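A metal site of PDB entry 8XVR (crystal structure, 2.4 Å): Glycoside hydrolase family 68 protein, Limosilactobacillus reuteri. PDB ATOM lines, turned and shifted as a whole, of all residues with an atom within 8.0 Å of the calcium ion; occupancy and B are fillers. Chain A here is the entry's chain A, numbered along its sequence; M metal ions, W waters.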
ATOM      1  N   GLN A 172      33.444  22.472 -20.201  1.00  0.00           N
ATOM      2  CA  GLN A 172      32.292  23.298 -19.789  1.00  0.00           C
ATOM      3  C   GLN A 172      31.651  22.623 -18.574  1.00  0.00           C
ATOM      4  O   GLN A 172      31.589  21.391 -18.468  1.00  0.00           O
ATOM      5  CB  GLN A 172      31.269  23.472 -20.915  1.00  0.00           C
ATOM      6  CG  GLN A 172      30.865  22.189 -21.632  1.00  0.00           C
ATOM      7  CD  GLN A 172      29.878  22.399 -22.760  1.00  0.00           C
ATOM      8  OE1 GLN A 172      28.955  23.175 -22.648  1.00  0.00           O
ATOM      9  NE2 GLN A 172      30.052  21.670 -23.850  1.00  0.00           N
ATOM     10  N   LYS A 194      33.234  18.179 -22.609  1.00  0.00           N
ATOM     11  CA  LYS A 194      34.342  18.920 -23.256  1.00  0.00           C
ATOM     12  C   LYS A 194      33.818  20.256 -23.753  1.00  0.00           C
ATOM     13  O   LYS A 194      32.733  20.313 -24.317  1.00  0.00           O
ATOM     14  CB  LYS A 194      34.946  18.133 -24.412  1.00  0.00           C
ATOM     15  CG  LYS A 194      35.776  16.927 -23.997  1.00  0.00           C
ATOM     16  CD  LYS A 194      36.482  16.335 -25.236  1.00  0.00           C
ATOM     17  CE  LYS A 194      37.283  15.074 -24.931  1.00  0.00           C
ATOM     18  NZ  LYS A 194      36.445  13.848 -25.112  1.00  0.00           N
ATOM     19  N   TYR A 195      34.574  21.315 -23.554  1.00  0.00           N
ATOM     20  CA  TYR A 195      34.176  22.628 -24.032  1.00  0.00           C
ATOM     21  C   TYR A 195      33.859  22.586 -25.514  1.00  0.00           C
ATOM     22  O   TYR A 195      34.671  22.135 -26.298  1.00  0.00           O
ATOM     23  CB  TYR A 195      35.270  23.671 -23.788  1.00  0.00           C
ATOM     24  CG  TYR A 195      34.742  25.065 -23.980  1.00  0.00           C
ATOM     25  CD1 TYR A 195      34.732  25.674 -25.250  1.00  0.00           C
ATOM     26  CD2 TYR A 195      34.210  25.776 -22.895  1.00  0.00           C
ATOM     27  CE1 TYR A 195      34.198  26.939 -25.437  1.00  0.00           C
ATOM     28  CE2 TYR A 195      33.692  27.042 -23.074  1.00  0.00           C
ATOM     29  CZ  TYR A 195      33.688  27.610 -24.346  1.00  0.00           C
ATOM     30  OH  TYR A 195      33.165  28.867 -24.515  1.00  0.00           O
ATOM     31  N   GLY A 196      32.647  23.034 -25.894  1.00  0.00           N
ATOM     32  CA  GLY A 196      32.214  23.118 -27.285  1.00  0.00           C
ATOM     33  C   GLY A 196      31.594  21.853 -27.832  1.00  0.00           C
ATOM     34  O   GLY A 196      31.110  21.840 -28.964  1.00  0.00           O
ATOM     35  N   ASP A 197      31.622  20.774 -27.062  1.00  0.00           N
ATOM     36  CA  ASP A 197      30.992  19.525 -27.432  1.00  0.00           C
ATOM     37  C   ASP A 197      29.489  19.751 -27.478  1.00  0.00           C
ATOM     38  O   ASP A 197      28.923  20.418 -26.602  1.00  0.00           O
ATOM     39  CB  ASP A 197      31.388  18.431 -26.435  1.00  0.00           C
ATOM     40  CG  ASP A 197      30.781  17.102 -26.745  1.00  0.00           C
ATOM     41  OD1 ASP A 197      29.519  16.982 -26.686  1.00  0.00           O
ATOM     42  OD2 ASP A 197      31.553  16.162 -27.057  1.00  0.00           O
ATOM     43  N   ASN A 198      28.844  19.194 -28.517  1.00  0.00           N
ATOM     44  CA  ASN A 198      27.449  19.491 -28.825  1.00  0.00           C
ATOM     45  C   ASN A 198      26.464  18.369 -28.533  1.00  0.00           C
ATOM     46  O   ASN A 198      25.268  18.478 -28.860  1.00  0.00           O
ATOM     47  CB  ASN A 198      27.328  19.900 -30.297  1.00  0.00           C
ATOM     48  CG  ASN A 198      27.969  21.242 -30.580  1.00  0.00           C
ATOM     49  OD1 ASN A 198      28.050  22.100 -29.705  1.00  0.00           O
ATOM     50  ND2 ASN A 198      28.409  21.452 -31.802  1.00  0.00           N
ATOM     51  N   GLU A 199      26.924  17.294 -27.894  1.00  0.00           N
ATOM     52  CA  GLU A 199      26.089  16.092 -27.749  1.00  0.00           C
ATOM     53  C   GLU A 199      25.498  16.005 -26.365  1.00  0.00           C
ATOM     54  O   GLU A 199      26.223  15.923 -25.358  1.00  0.00           O
ATOM     55  CB  GLU A 199      26.895  14.811 -28.039  1.00  0.00           C
ATOM     56  CG  GLU A 199      27.483  14.705 -29.442  1.00  0.00           C
ATOM     57  CD  GLU A 199      26.422  14.756 -30.532  1.00  0.00           C
ATOM     58  OE1 GLU A 199      25.336  14.141 -30.359  1.00  0.00           O
ATOM     59  OE2 GLU A 199      26.668  15.423 -31.564  1.00  0.00           O
ATOM     60  N   LEU A 495      21.926  33.257 -26.654  1.00  0.00           N
ATOM     61  CA  LEU A 495      21.450  31.885 -26.821  1.00  0.00           C
ATOM     62  C   LEU A 495      20.462  31.594 -25.678  1.00  0.00           C
ATOM     63  O   LEU A 495      20.809  31.724 -24.500  1.00  0.00           O
ATOM     64  CB  LEU A 495      22.628  30.935 -26.776  1.00  0.00           C
ATOM     65  CG  LEU A 495      22.309  29.452 -26.944  1.00  0.00           C
ATOM     66  CD1 LEU A 495      21.828  29.170 -28.353  1.00  0.00           C
ATOM     67  CD2 LEU A 495      23.563  28.648 -26.601  1.00  0.00           C
ATOM     68  N   THR A 536      19.999  24.625 -31.758  1.00  0.00           N
ATOM     69  CA  THR A 536      21.071  23.675 -31.437  1.00  0.00           C
ATOM     70  C   THR A 536      20.521  22.294 -31.094  1.00  0.00           C
ATOM     71  O   THR A 536      19.316  22.095 -30.997  1.00  0.00           O
ATOM     72  CB  THR A 536      21.878  24.132 -30.190  1.00  0.00           C
ATOM     73  OG1 THR A 536      21.074  23.977 -29.002  1.00  0.00           O
ATOM     74  CG2 THR A 536      22.295  25.563 -30.316  1.00  0.00           C
ATOM     75  N   ASN A 537      21.418  21.368 -30.824  1.00  0.00           N
ATOM     76  CA  ASN A 537      21.037  20.143 -30.103  1.00  0.00           C
ATOM     77  C   ASN A 537      20.516  20.456 -28.711  1.00  0.00           C
ATOM     78  O   ASN A 537      20.664  21.550 -28.214  1.00  0.00           O
ATOM     79  CB  ASN A 537      22.239  19.212 -29.951  1.00  0.00           C
ATOM     80  CG  ASN A 537      22.566  18.441 -31.213  1.00  0.00           C
ATOM     81  OD1 ASN A 537      21.692  18.080 -31.985  1.00  0.00           O
ATOM     82  ND2 ASN A 537      23.825  18.152 -31.404  1.00  0.00           N
ATOM     83  N   GLY A 539      20.619  20.805 -24.919  1.00  0.00           N
ATOM     84  CA  GLY A 539      21.639  21.015 -23.853  1.00  0.00           C
ATOM     85  C   GLY A 539      22.911  21.681 -24.348  1.00  0.00           C
ATOM     86  O   GLY A 539      23.977  21.483 -23.764  1.00  0.00           O
ATOM     87  N   ASP A 540      22.802  22.429 -25.457  1.00  0.00           N
ATOM     88  CA  ASP A 540      23.887  23.243 -25.954  1.00  0.00           C
ATOM     89  C   ASP A 540      23.859  24.625 -25.255  1.00  0.00           C
ATOM     90  O   ASP A 540      22.894  25.387 -25.381  1.00  0.00           O
ATOM     91  CB  ASP A 540      23.762  23.409 -27.466  1.00  0.00           C
ATOM     92  CG  ASP A 540      25.080  23.835 -28.134  1.00  0.00           C
ATOM     93  OD1 ASP A 540      25.941  24.475 -27.486  1.00  0.00           O
ATOM     94  OD2 ASP A 540      25.233  23.542 -29.347  1.00  0.00           O
ATOM     95  N   TRP A 541      24.941  24.932 -24.540  1.00  0.00           N
ATOM     96  CA  TRP A 541      25.163  26.191 -23.838  1.00  0.00           C
ATOM     97  C   TRP A 541      26.036  27.167 -24.621  1.00  0.00           C
ATOM     98  O   TRP A 541      26.173  28.331 -24.237  1.00  0.00           O
ATOM     99  CB  TRP A 541      25.831  25.898 -22.467  1.00  0.00           C
ATOM    100  CG  TRP A 541      25.000  24.994 -21.682  1.00  0.00           C
ATOM    101  CD1 TRP A 541      25.041  23.650 -21.693  1.00  0.00           C
ATOM    102  CD2 TRP A 541      23.930  25.360 -20.816  1.00  0.00           C
ATOM    103  NE1 TRP A 541      24.084  23.126 -20.871  1.00  0.00           N
ATOM    104  CE2 TRP A 541      23.371  24.148 -20.324  1.00  0.00           C
ATOM    105  CE3 TRP A 541      23.387  26.578 -20.397  1.00  0.00           C
ATOM    106  CZ2 TRP A 541      22.293  24.129 -19.423  1.00  0.00           C
ATOM    107  CZ3 TRP A 541      22.313  26.568 -19.507  1.00  0.00           C
ATOM    108  CH2 TRP A 541      21.774  25.338 -19.031  1.00  0.00           C
ATOM    109  N   ILE A 542      26.632  26.676 -25.716  1.00  0.00           N
ATOM    110  CA  ILE A 542      27.673  27.417 -26.433  1.00  0.00           C
ATOM    111  C   ILE A 542      27.353  27.484 -27.924  1.00  0.00           C
ATOM    112  O   ILE A 542      27.526  26.517 -28.665  1.00  0.00           O
ATOM    113  CB  ILE A 542      29.050  26.743 -26.228  1.00  0.00           C
ATOM    114  CG1 ILE A 542      29.409  26.661 -24.732  1.00  0.00           C
ATOM    115  CG2 ILE A 542      30.150  27.470 -27.018  1.00  0.00           C
ATOM    116  CD1 ILE A 542      30.567  25.727 -24.435  1.00  0.00           C
ATOM    117  N   TRP A 543      26.910  28.629 -28.377  1.00  0.00           N
ATOM    118  CA  TRP A 543      26.592  28.791 -29.776  1.00  0.00           C
ATOM    119  C   TRP A 543      27.835  29.042 -30.609  1.00  0.00           C
ATOM    120  O   TRP A 543      28.649  29.844 -30.277  1.00  0.00           O
ATOM    121  CB  TRP A 543      25.603  29.950 -30.000  1.00  0.00           C
ATOM    122  CG  TRP A 543      25.362  30.108 -31.474  1.00  0.00           C
ATOM    123  CD1 TRP A 543      26.045  30.947 -32.314  1.00  0.00           C
ATOM    124  CD2 TRP A 543      24.471  29.352 -32.286  1.00  0.00           C
ATOM    125  NE1 TRP A 543      25.590  30.776 -33.597  1.00  0.00           N
ATOM    126  CE2 TRP A 543      24.624  29.812 -33.606  1.00  0.00           C
ATOM    127  CE3 TRP A 543      23.525  28.360 -32.023  1.00  0.00           C
ATOM    128  CZ2 TRP A 543      23.897  29.287 -34.686  1.00  0.00           C
ATOM    129  CZ3 TRP A 543      22.774  27.832 -33.107  1.00  0.00           C
ATOM    130  CH2 TRP A 543      22.990  28.302 -34.409  1.00  0.00           C
ATOM    131  N   ASP A 544      27.946  28.340 -31.725  1.00  0.00           N
ATOM    132  CA  ASP A 544      28.891  28.684 -32.795  1.00  0.00           C
ATOM    133  C   ASP A 544      28.334  28.123 -34.102  1.00  0.00           C
ATOM    134  O   ASP A 544      27.214  27.609 -34.125  1.00  0.00           O
ATOM    135  CB  ASP A 544      30.309  28.196 -32.471  1.00  0.00           C
ATOM    136  CG  ASP A 544      30.364  26.709 -32.104  1.00  0.00           C
ATOM    137  OD1 ASP A 544      29.593  25.902 -32.706  1.00  0.00           O
ATOM    138  OD2 ASP A 544      31.183  26.371 -31.223  1.00  0.00           O
ATOM    139  N   ASP A 545      29.053  28.287 -35.204  1.00  0.00           N
ATOM    140  CA  ASP A 545      28.495  27.878 -36.521  1.00  0.00           C
ATOM    141  C   ASP A 545      28.226  26.380 -36.540  1.00  0.00           C
ATOM    142  O   ASP A 545      27.119  25.982 -36.892  1.00  0.00           O
ATOM    143  CB  ASP A 545      29.424  28.316 -37.655  1.00  0.00           C
ATOM    144  CG  ASP A 545      29.402  29.849 -37.859  1.00  0.00           C
ATOM    145  OD1 ASP A 545      28.296  30.483 -37.816  1.00  0.00           O
ATOM    146  OD2 ASP A 545      30.519  30.392 -38.069  1.00  0.00           O
ATOM    147  N   SER A 546      29.225  25.632 -36.072  1.00  0.00           N
ATOM    148  CA  SER A 546      29.150  24.168 -35.854  1.00  0.00           C
ATOM    149  C   SER A 546      27.932  23.683 -35.021  1.00  0.00           C
ATOM    150  O   SER A 546      27.620  22.525 -35.058  1.00  0.00           O
ATOM    151  CB  SER A 546      30.474  23.657 -35.190  1.00  0.00           C
ATOM    152  OG  SER A 546      30.380  23.578 -33.725  1.00  0.00           O
ATOM    153  N   SER A 547      27.281  24.551 -34.242  1.00  0.00           N
ATOM    154  CA  SER A 547      26.269  24.088 -33.295  1.00  0.00           C
ATOM    155  C   SER A 547      24.835  23.934 -33.857  1.00  0.00           C
ATOM    156  O   SER A 547      24.015  23.279 -33.229  1.00  0.00           O
ATOM    157  CB  SER A 547      26.211  25.008 -32.067  1.00  0.00           C
ATOM    158  OG  SER A 547      27.357  24.881 -31.257  1.00  0.00           O
ATOM    159  N   GLU A 548      24.557  24.505 -35.017  1.00  0.00           N
ATOM    160  CA  GLU A 548      23.224  24.476 -35.574  1.00  0.00           C
ATOM    161  C   GLU A 548      22.822  23.076 -36.025  1.00  0.00           C
ATOM    162  O   GLU A 548      23.604  22.365 -36.650  1.00  0.00           O
ATOM    163  CB  GLU A 548      23.068  25.447 -36.712  1.00  0.00           C
ATOM    164  CG  GLU A 548      21.621  25.627 -37.134  1.00  0.00           C
ATOM    165  CD  GLU A 548      21.448  26.827 -38.065  1.00  0.00           C
ATOM    166  OE1 GLU A 548      22.393  27.638 -38.215  1.00  0.00           O
ATOM    167  OE2 GLU A 548      20.366  26.974 -38.680  1.00  0.00           O
HETATM  168 CA    CA M   1      27.649  24.247 -29.041  1.00  0.00          CA
HETATM  169  O   HOH W   1      28.753  23.245 -27.213  1.00  0.00           O
HETATM  170  O   HOH W   2      29.899  24.454 -29.492  1.00  0.00           O
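The side-chain amide oxygen (OD1) of Asn 198 binds the calcium ion (2.3 Å).
O of Ile 542 is bound to the calcium ion (2.3 Å).
Water W2 is bound to the calcium ion.
OD1 of Asp 540 is bound to the calcium ion (2.3 Å).
The side-chain hydroxyl (OG) of Ser 547 binds the calcium ion (2.3 Å).
The calcium ion is bound by water W1 (2.4 Å).
The side-chain carboxylate (OD2) of Asp 540 is bound to the calcium ion (2.5 Å).
The calcium ion has seven donor atoms within binding distance.
Water W2 bridges the side-chain carboxylate of Asp 544 (2.9 Å) and the backbone carbonyl oxygen of Gly 196 (2.9 Å).
The side-chain amide oxygen (OD1) of Asn 198 sits close to the backbone carbonyl oxygen (O) of Gly 196, at 3.2 Å.
ND2 of Asn 198 lies within hydrogen-bond range of OG of Ser 546 (3.5 Å).
O of Asn 198 lies within hydrogen-bond range of ND2 of Asn 537 (2.9 Å).
OD1 of Asp 544 is in hydrogen-bond range of N of Ser 547 (3.1 Å).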
